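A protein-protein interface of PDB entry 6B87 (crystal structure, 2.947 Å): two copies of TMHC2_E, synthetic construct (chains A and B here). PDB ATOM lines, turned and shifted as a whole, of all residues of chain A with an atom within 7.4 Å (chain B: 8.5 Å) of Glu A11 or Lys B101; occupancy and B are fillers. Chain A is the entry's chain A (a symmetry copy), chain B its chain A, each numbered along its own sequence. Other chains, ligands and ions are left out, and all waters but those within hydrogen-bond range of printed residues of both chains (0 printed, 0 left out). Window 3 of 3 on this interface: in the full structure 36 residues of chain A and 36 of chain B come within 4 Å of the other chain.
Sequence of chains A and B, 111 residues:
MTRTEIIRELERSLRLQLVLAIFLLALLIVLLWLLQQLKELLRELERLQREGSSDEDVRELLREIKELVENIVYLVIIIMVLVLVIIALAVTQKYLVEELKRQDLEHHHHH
Glu A11 touches just one residue of chain B: Lys B101.
Arg A12 touches none of the printed residues of chain B.
Printed residues of chain B within 4 Å of Leu A14: Gln B93 (3.3 Å), Lys B94 (3.9 Å) and Val B97 (3.7 Å).
Of the printed residues of chain B, Gln A93 touches Gln B93.
Of the printed residues of chain A, Gln B93 touches Leu A14 (3.3 Å) and Gln A93 (3.6 Å).
Printed residues of chain A within 4 Å of Lys B94: Leu A14 (3.9 Å).
Leu B96 touches none of the printed residues of chain A.
Of the printed residues of chain A, Val B97 touches Leu A14 (3.7 Å).
Of chain A, only Glu A11 (2.8 Å) comes within 4 Å of Lys B101.
Gln B93 touches its own counterpart, Gln A93.
3 positions are printed for both chains.
Of the 5 pairs that touch across the chains among the printed residues, 1 has its exchanged pair printed and touching as well.
The side-chain carboxylate of Glu A11 is in salt-bridge range of the side-chain amino group of Lys B101, 2.8 Å away.
The side-chain carboxylate (OE2) of Glu A11 is in salt-bridge range of the guanidinium group (NH2) of Arg A15 (2.8 Å).
The side-chain amide nitrogen (NE2) of Gln A93 is in hydrogen-bond range of the side-chain hydroxyl (OG) of Ser A13, 2.9 Å away.
The side-chain amide nitrogen (NE2) of Gln A93 sits at hydrogen-bond distance from the side-chain amide oxygen (OE1) of Gln A17 (3.3 Å).
Among the printed residues, pairs that only touch across the chains: Leu A14 with Gln B93, Gln A93 with Gln B93, Leu A14 with Val B97 and Leu A14 with Lys B94.
Of the 14 printed residues of chain B, 4 touch a printed residue of chain A.
Printed residues of chain B that touch a printed residue of chain A: Gln B93, Lys B94, Val B97 and Lys B101.
Among the printed residues, Asp or Glu carboxylates within 4 Å of a Lys or Arg side-chain nitrogen of the other chain: Glu A11 with Lys B101 (2.8 Å).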
ATOM      1  N   GLU A   5      16.358  -9.417  -5.800  1.00  0.00           N
ATOM      2  CA  GLU A   5      17.547  -9.821  -5.047  1.00  0.00           C
ATOM      3  C   GLU A   5      18.182 -11.077  -5.640  1.00  0.00           C
ATOM      4  O   GLU A   5      19.404 -11.227  -5.607  1.00  0.00           O
ATOM      5  CB  GLU A   5      17.191 -10.061  -3.587  1.00  0.00           C
ATOM      6  N   ILE A   6      17.346 -11.970  -6.170  1.00  0.00           N
ATOM      7  CA  ILE A   6      17.794 -13.189  -6.820  1.00  0.00           C
ATOM      8  C   ILE A   6      18.165 -12.900  -8.273  1.00  0.00           C
ATOM      9  O   ILE A   6      19.290 -13.128  -8.730  1.00  0.00           O
ATOM     10  CB  ILE A   6      16.686 -14.265  -6.785  1.00  0.00           C
ATOM     11  CG1 ILE A   6      16.329 -14.666  -5.348  1.00  0.00           C
ATOM     12  CG2 ILE A   6      17.122 -15.468  -7.580  1.00  0.00           C
ATOM     13  CD1 ILE A   6      15.104 -15.569  -5.264  1.00  0.00           C
ATOM     14  N   ARG A   8      20.163 -10.395  -8.700  1.00  0.00           N
ATOM     15  CA  ARG A   8      21.498  -9.958  -8.332  1.00  0.00           C
ATOM     16  C   ARG A   8      22.372 -11.133  -7.901  1.00  0.00           C
ATOM     17  O   ARG A   8      23.487 -11.291  -8.406  1.00  0.00           O
ATOM     18  CB  ARG A   8      21.417  -8.926  -7.220  1.00  0.00           C
ATOM     19  N   GLU A   9      21.865 -11.939  -6.960  1.00  0.00           N
ATOM     20  CA  GLU A   9      22.608 -13.066  -6.404  1.00  0.00           C
ATOM     21  C   GLU A   9      22.974 -14.093  -7.469  1.00  0.00           C
ATOM     22  O   GLU A   9      24.107 -14.577  -7.474  1.00  0.00           O
ATOM     23  CB  GLU A   9      21.800 -13.735  -5.301  1.00  0.00           C
ATOM     24  N   LEU A  10      22.037 -14.408  -8.382  1.00  0.00           N
ATOM     25  CA  LEU A  10      22.338 -15.337  -9.474  1.00  0.00           C
ATOM     26  C   LEU A  10      23.417 -14.826 -10.384  1.00  0.00           C
ATOM     27  O   LEU A  10      24.255 -15.612 -10.817  1.00  0.00           O
ATOM     28  CB  LEU A  10      21.105 -15.649 -10.334  1.00  0.00           C
ATOM     29  CG  LEU A  10      20.093 -16.649  -9.765  1.00  0.00           C
ATOM     30  CD1 LEU A  10      18.834 -16.652 -10.622  1.00  0.00           C
ATOM     31  CD2 LEU A  10      20.724 -18.033  -9.793  1.00  0.00           C
ATOM     32  N   GLU A  11      23.416 -13.530 -10.682  1.00  0.00           N
ATOM     33  CA  GLU A  11      24.457 -12.990 -11.536  1.00  0.00           C
ATOM     34  C   GLU A  11      25.818 -13.100 -10.867  1.00  0.00           C
ATOM     35  O   GLU A  11      26.787 -13.513 -11.496  1.00  0.00           O
ATOM     36  CB  GLU A  11      24.215 -11.539 -11.908  1.00  0.00           C
ATOM     37  CG  GLU A  11      25.296 -11.034 -12.851  1.00  0.00           C
ATOM     38  CD  GLU A  11      25.203  -9.578 -13.195  1.00  0.00           C
ATOM     39  OE1 GLU A  11      24.442  -9.227 -14.065  1.00  0.00           O
ATOM     40  OE2 GLU A  11      25.926  -8.812 -12.593  1.00  0.00           O
ATOM     41  N   ARG A  12      25.893 -12.734  -9.597  1.00  0.00           N
ATOM     42  CA  ARG A  12      27.151 -12.817  -8.883  1.00  0.00           C
ATOM     43  C   ARG A  12      27.655 -14.234  -8.777  1.00  0.00           C
ATOM     44  O   ARG A  12      28.854 -14.487  -8.927  1.00  0.00           O
ATOM     45  CB  ARG A  12      27.020 -12.247  -7.494  1.00  0.00           C
ATOM     46  CG  ARG A  12      26.952 -10.739  -7.424  1.00  0.00           C
ATOM     47  CD  ARG A  12      27.123 -10.282  -6.023  1.00  0.00           C
ATOM     48  NE  ARG A  12      25.964 -10.595  -5.205  1.00  0.00           N
ATOM     49  CZ  ARG A  12      24.918  -9.763  -5.033  1.00  0.00           C
ATOM     50  NH1 ARG A  12      24.924  -8.587  -5.623  1.00  0.00           N
ATOM     51  NH2 ARG A  12      23.904 -10.127  -4.265  1.00  0.00           N
ATOM     52  N   SER A  13      26.743 -15.158  -8.518  1.00  0.00           N
ATOM     53  CA  SER A  13      27.096 -16.555  -8.409  1.00  0.00           C
ATOM     54  C   SER A  13      27.631 -17.085  -9.741  1.00  0.00           C
ATOM     55  O   SER A  13      28.628 -17.813  -9.771  1.00  0.00           O
ATOM     56  CB  SER A  13      25.890 -17.339  -7.960  1.00  0.00           C
ATOM     57  OG  SER A  13      26.213 -18.687  -7.790  1.00  0.00           O
ATOM     58  N   LEU A  14      26.967 -16.697 -10.835  1.00  0.00           N
ATOM     59  CA  LEU A  14      27.386 -17.049 -12.184  1.00  0.00           C
ATOM     60  C   LEU A  14      28.697 -16.409 -12.567  1.00  0.00           C
ATOM     61  O   LEU A  14      29.505 -17.049 -13.236  1.00  0.00           O
ATOM     62  CB  LEU A  14      26.300 -16.662 -13.189  1.00  0.00           C
ATOM     63  CG  LEU A  14      25.042 -17.547 -13.158  1.00  0.00           C
ATOM     64  CD1 LEU A  14      23.939 -16.927 -13.998  1.00  0.00           C
ATOM     65  CD2 LEU A  14      25.409 -18.905 -13.706  1.00  0.00           C
ATOM     66  N   ARG A  15      28.945 -15.178 -12.106  1.00  0.00           N
ATOM     67  CA  ARG A  15      30.243 -14.541 -12.304  1.00  0.00           C
ATOM     68  C   ARG A  15      31.353 -15.391 -11.697  1.00  0.00           C
ATOM     69  O   ARG A  15      32.375 -15.619 -12.347  1.00  0.00           O
ATOM     70  CB  ARG A  15      30.277 -13.146 -11.676  1.00  0.00           C
ATOM     71  CG  ARG A  15      29.508 -12.053 -12.408  1.00  0.00           C
ATOM     72  CD  ARG A  15      29.535 -10.765 -11.655  1.00  0.00           C
ATOM     73  NE  ARG A  15      28.752  -9.736 -12.319  1.00  0.00           N
ATOM     74  CZ  ARG A  15      29.186  -8.974 -13.338  1.00  0.00           C
ATOM     75  NH1 ARG A  15      30.400  -9.124 -13.821  1.00  0.00           N
ATOM     76  NH2 ARG A  15      28.366  -8.074 -13.846  1.00  0.00           N
ATOM     77  N   LEU A  16      31.131 -15.898 -10.474  1.00  0.00           N
ATOM     78  CA  LEU A  16      32.100 -16.799  -9.866  1.00  0.00           C
ATOM     79  C   LEU A  16      32.294 -18.092 -10.608  1.00  0.00           C
ATOM     80  O   LEU A  16      33.438 -18.466 -10.860  1.00  0.00           O
ATOM     81  CB  LEU A  16      31.732 -17.153  -8.432  1.00  0.00           C
ATOM     82  CG  LEU A  16      32.111 -16.142  -7.379  1.00  0.00           C
ATOM     83  CD1 LEU A  16      31.493 -16.557  -6.053  1.00  0.00           C
ATOM     84  CD2 LEU A  16      33.630 -16.106  -7.291  1.00  0.00           C
ATOM     85  N   GLN A  17      31.209 -18.781 -10.972  1.00  0.00           N
ATOM     86  CA  GLN A  17      31.416 -20.037 -11.668  1.00  0.00           C
ATOM     87  C   GLN A  17      32.120 -19.893 -12.966  1.00  0.00           C
ATOM     88  O   GLN A  17      32.928 -20.750 -13.305  1.00  0.00           O
ATOM     89  CB  GLN A  17      30.156 -20.775 -12.002  1.00  0.00           C
ATOM     90  CG  GLN A  17      29.463 -21.490 -10.898  1.00  0.00           C
ATOM     91  CD  GLN A  17      28.400 -22.334 -11.534  1.00  0.00           C
ATOM     92  OE1 GLN A  17      27.808 -21.903 -12.530  1.00  0.00           O
ATOM     93  NE2 GLN A  17      28.172 -23.531 -11.028  1.00  0.00           N
ATOM     94  N   GLN A  93      22.577 -21.936  -7.239  1.00  0.00           N
ATOM     95  CA  GLN A  93      21.823 -21.354  -8.332  1.00  0.00           C
ATOM     96  C   GLN A  93      20.537 -22.100  -8.600  1.00  0.00           C
ATOM     97  O   GLN A  93      19.516 -21.474  -8.872  1.00  0.00           O
ATOM     98  CB  GLN A  93      22.680 -21.345  -9.575  1.00  0.00           C
ATOM     99  CG  GLN A  93      23.836 -20.385  -9.488  1.00  0.00           C
ATOM    100  CD  GLN A  93      24.885 -20.664 -10.531  1.00  0.00           C
ATOM    101  OE1 GLN A  93      24.648 -21.345 -11.531  1.00  0.00           O
ATOM    102  NE2 GLN A  93      26.068 -20.138 -10.291  1.00  0.00           N
ATOM    103  N   LEU A  96      18.105 -21.050  -5.955  1.00  0.00           N
ATOM    104  CA  LEU A  96      17.661 -19.684  -6.230  1.00  0.00           C
ATOM    105  C   LEU A  96      16.581 -19.649  -7.300  1.00  0.00           C
ATOM    106  O   LEU A  96      15.576 -18.955  -7.143  1.00  0.00           O
ATOM    107  CB  LEU A  96      18.855 -18.821  -6.677  1.00  0.00           C
ATOM    108  CG  LEU A  96      19.872 -18.416  -5.592  1.00  0.00           C
ATOM    109  CD1 LEU A  96      21.093 -17.775  -6.245  1.00  0.00           C
ATOM    110  CD2 LEU A  96      19.222 -17.439  -4.630  1.00  0.00           C
ATOM    111  N   ILE B   6      12.456 -18.019 -19.364  1.00  0.00           N
ATOM    112  CA  ILE B   6      13.801 -18.024 -18.818  1.00  0.00           C
ATOM    113  C   ILE B   6      13.781 -18.553 -17.386  1.00  0.00           C
ATOM    114  O   ILE B   6      14.436 -19.538 -17.032  1.00  0.00           O
ATOM    115  CB  ILE B   6      14.396 -16.598 -18.823  1.00  0.00           C
ATOM    116  CG1 ILE B   6      14.527 -16.042 -20.247  1.00  0.00           C
ATOM    117  CG2 ILE B   6      15.734 -16.605 -18.131  1.00  0.00           C
ATOM    118  CD1 ILE B   6      14.915 -14.569 -20.283  1.00  0.00           C
ATOM    119  N   ALA B  90      27.503 -22.214 -18.633  1.00  0.00           N
ATOM    120  CA  ALA B  90      27.624 -21.072 -17.716  1.00  0.00           C
ATOM    121  C   ALA B  90      27.411 -19.759 -18.430  1.00  0.00           C
ATOM    122  O   ALA B  90      26.735 -18.869 -17.907  1.00  0.00           O
ATOM    123  CB  ALA B  90      28.986 -21.047 -17.047  1.00  0.00           C
ATOM    124  N   GLN B  93      23.690 -19.283 -19.250  1.00  0.00           N
ATOM    125  CA  GLN B  93      22.963 -18.855 -18.071  1.00  0.00           C
ATOM    126  C   GLN B  93      23.211 -17.402 -17.743  1.00  0.00           C
ATOM    127  O   GLN B  93      22.282 -16.697 -17.358  1.00  0.00           O
ATOM    128  CB  GLN B  93      23.363 -19.721 -16.902  1.00  0.00           C
ATOM    129  CG  GLN B  93      22.882 -21.142 -17.027  1.00  0.00           C
ATOM    130  CD  GLN B  93      23.604 -22.070 -16.087  1.00  0.00           C
ATOM    131  OE1 GLN B  93      24.229 -21.654 -15.109  1.00  0.00           O
ATOM    132  NE2 GLN B  93      23.525 -23.349 -16.391  1.00  0.00           N
ATOM    133  N   LYS B  94      24.456 -16.946 -17.911  1.00  0.00           N
ATOM    134  CA  LYS B  94      24.790 -15.552 -17.672  1.00  0.00           C
ATOM    135  C   LYS B  94      24.013 -14.639 -18.608  1.00  0.00           C
ATOM    136  O   LYS B  94      23.480 -13.618 -18.172  1.00  0.00           O
ATOM    137  CB  LYS B  94      26.281 -15.334 -17.844  1.00  0.00           C
ATOM    138  N   TYR B  95      23.929 -15.020 -19.884  1.00  0.00           N
ATOM    139  CA  TYR B  95      23.180 -14.255 -20.877  1.00  0.00           C
ATOM    140  C   TYR B  95      21.680 -14.245 -20.578  1.00  0.00           C
ATOM    141  O   TYR B  95      21.027 -13.211 -20.730  1.00  0.00           O
ATOM    142  CB  TYR B  95      23.430 -14.820 -22.262  1.00  0.00           C
ATOM    143  N   LEU B  96      21.147 -15.385 -20.127  1.00  0.00           N
ATOM    144  CA  LEU B  96      19.739 -15.488 -19.745  1.00  0.00           C
ATOM    145  C   LEU B  96      19.401 -14.555 -18.593  1.00  0.00           C
ATOM    146  O   LEU B  96      18.380 -13.867 -18.632  1.00  0.00           O
ATOM    147  CB  LEU B  96      19.405 -16.937 -19.348  1.00  0.00           C
ATOM    148  CG  LEU B  96      19.312 -17.972 -20.486  1.00  0.00           C
ATOM    149  CD1 LEU B  96      19.209 -19.376 -19.899  1.00  0.00           C
ATOM    150  CD2 LEU B  96      18.092 -17.674 -21.340  1.00  0.00           C
ATOM    151  N   VAL B  97      20.281 -14.502 -17.596  1.00  0.00           N
ATOM    152  CA  VAL B  97      20.114 -13.602 -16.471  1.00  0.00           C
ATOM    153  C   VAL B  97      20.287 -12.145 -16.872  1.00  0.00           C
ATOM    154  O   VAL B  97      19.570 -11.285 -16.367  1.00  0.00           O
ATOM    155  CB  VAL B  97      21.079 -13.963 -15.348  1.00  0.00           C
ATOM    156  CG1 VAL B  97      21.041 -12.887 -14.276  1.00  0.00           C
ATOM    157  CG2 VAL B  97      20.662 -15.306 -14.762  1.00  0.00           C
ATOM    158  N   GLU B  98      21.230 -11.863 -17.775  1.00  0.00           N
ATOM    159  CA  GLU B  98      21.397 -10.512 -18.307  1.00  0.00           C
ATOM    160  C   GLU B  98      20.122 -10.009 -19.018  1.00  0.00           C
ATOM    161  O   GLU B  98      19.663  -8.898 -18.761  1.00  0.00           O
ATOM    162  CB  GLU B  98      22.595 -10.458 -19.261  1.00  0.00           C
ATOM    163  CG  GLU B  98      22.855  -9.087 -19.876  1.00  0.00           C
ATOM    164  CD  GLU B  98      24.087  -9.048 -20.746  1.00  0.00           C
ATOM    165  OE1 GLU B  98      24.899  -9.933 -20.626  1.00  0.00           O
ATOM    166  OE2 GLU B  98      24.221  -8.131 -21.529  1.00  0.00           O
ATOM    167  N   GLU B  99      19.534 -10.830 -19.888  1.00  0.00           N
ATOM    168  CA  GLU B  99      18.297 -10.435 -20.565  1.00  0.00           C
ATOM    169  C   GLU B  99      17.113 -10.344 -19.606  1.00  0.00           C
ATOM    170  O   GLU B  99      16.222  -9.505 -19.786  1.00  0.00           O
ATOM    171  CB  GLU B  99      17.979 -11.400 -21.698  1.00  0.00           C
ATOM    172  CG  GLU B  99      18.887 -11.247 -22.910  1.00  0.00           C
ATOM    173  CD  GLU B  99      18.704  -9.918 -23.598  1.00  0.00           C
ATOM    174  OE1 GLU B  99      17.580  -9.566 -23.870  1.00  0.00           O
ATOM    175  OE2 GLU B  99      19.682  -9.252 -23.844  1.00  0.00           O
ATOM    176  N   LEU B 100      17.125 -11.186 -18.582  1.00  0.00           N
ATOM    177  CA  LEU B 100      16.132 -11.151 -17.530  1.00  0.00           C
ATOM    178  C   LEU B 100      16.221  -9.854 -16.703  1.00  0.00           C
ATOM    179  O   LEU B 100      15.202  -9.224 -16.421  1.00  0.00           O
ATOM    180  CB  LEU B 100      16.321 -12.382 -16.647  1.00  0.00           C
ATOM    181  CG  LEU B 100      15.325 -12.578 -15.517  1.00  0.00           C
ATOM    182  CD1 LEU B 100      13.931 -12.680 -16.110  1.00  0.00           C
ATOM    183  CD2 LEU B 100      15.692 -13.848 -14.758  1.00  0.00           C
ATOM    184  N   LYS B 101      17.441  -9.436 -16.327  1.00  0.00           N
ATOM    185  CA  LYS B 101      17.600  -8.199 -15.553  1.00  0.00           C
ATOM    186  C   LYS B 101      17.316  -6.943 -16.380  1.00  0.00           C
ATOM    187  O   LYS B 101      17.063  -5.883 -15.810  1.00  0.00           O
ATOM    188  CB  LYS B 101      18.999  -8.071 -14.929  1.00  0.00           C
ATOM    189  CG  LYS B 101      20.120  -7.782 -15.906  1.00  0.00           C
ATOM    190  CD  LYS B 101      21.445  -7.543 -15.203  1.00  0.00           C
ATOM    191  CE  LYS B 101      22.543  -7.167 -16.190  1.00  0.00           C
ATOM    192  NZ  LYS B 101      23.830  -6.876 -15.495  1.00  0.00           N
ATOM    193  N   ARG B 102      17.303  -7.058 -17.716  1.00  0.00           N
ATOM    194  CA  ARG B 102      16.898  -5.944 -18.576  1.00  0.00           C
ATOM    195  C   ARG B 102      15.394  -5.608 -18.540  1.00  0.00           C
ATOM    196  O   ARG B 102      14.966  -4.667 -19.213  1.00  0.00           O
ATOM    197  CB  ARG B 102      17.296  -6.213 -20.015  1.00  0.00           C
ATOM    198  CG  ARG B 102      18.788  -6.143 -20.260  1.00  0.00           C
ATOM    199  CD  ARG B 102      19.167  -6.484 -21.652  1.00  0.00           C
ATOM    200  NE  ARG B 102      20.610  -6.569 -21.776  1.00  0.00           N
ATOM    201  CZ  ARG B 102      21.435  -5.512 -21.874  1.00  0.00           C
ATOM    202  NH1 ARG B 102      20.940  -4.292 -21.877  1.00  0.00           N
ATOM    203  NH2 ARG B 102      22.742  -5.694 -21.961  1.00  0.00           N
ATOM    204  N   GLN B 103      14.601  -6.325 -17.738  1.00  0.00           N
ATOM    205  CA  GLN B 103      13.196  -5.993 -17.589  1.00  0.00           C
ATOM    206  C   GLN B 103      13.027  -4.994 -16.430  1.00  0.00           C
ATOM    207  O   GLN B 103      13.872  -4.928 -15.537  1.00  0.00           O
ATOM    208  CB  GLN B 103      12.391  -7.261 -17.338  1.00  0.00           C
ATOM    209  CG  GLN B 103      12.666  -8.358 -18.361  1.00  0.00           C
ATOM    210  CD  GLN B 103      12.459  -7.919 -19.795  1.00  0.00           C
ATOM    211  OE1 GLN B 103      11.394  -7.412 -20.158  1.00  0.00           O
ATOM    212  NE2 GLN B 103      13.481  -8.115 -20.625  1.00  0.00           N
ATOM    213  N   ASP B 104      11.955  -4.198 -16.460  1.00  0.00           N
ATOM    214  CA  ASP B 104      11.731  -3.142 -15.441  1.00  0.00           C
ATOM    215  C   ASP B 104      11.729  -3.649 -13.995  1.00  0.00           C
ATOM    216  O   ASP B 104      12.400  -3.061 -13.142  1.00  0.00           O
ATOM    217  CB  ASP B 104      10.402  -2.403 -15.695  1.00  0.00           C
ATOM    218  CG  ASP B 104      10.182  -1.195 -14.763  1.00  0.00           C
ATOM    219  OD1 ASP B 104      10.663  -0.129 -15.073  1.00  0.00           O
ATOM    220  OD2 ASP B 104       9.527  -1.352 -13.759  1.00  0.00           O
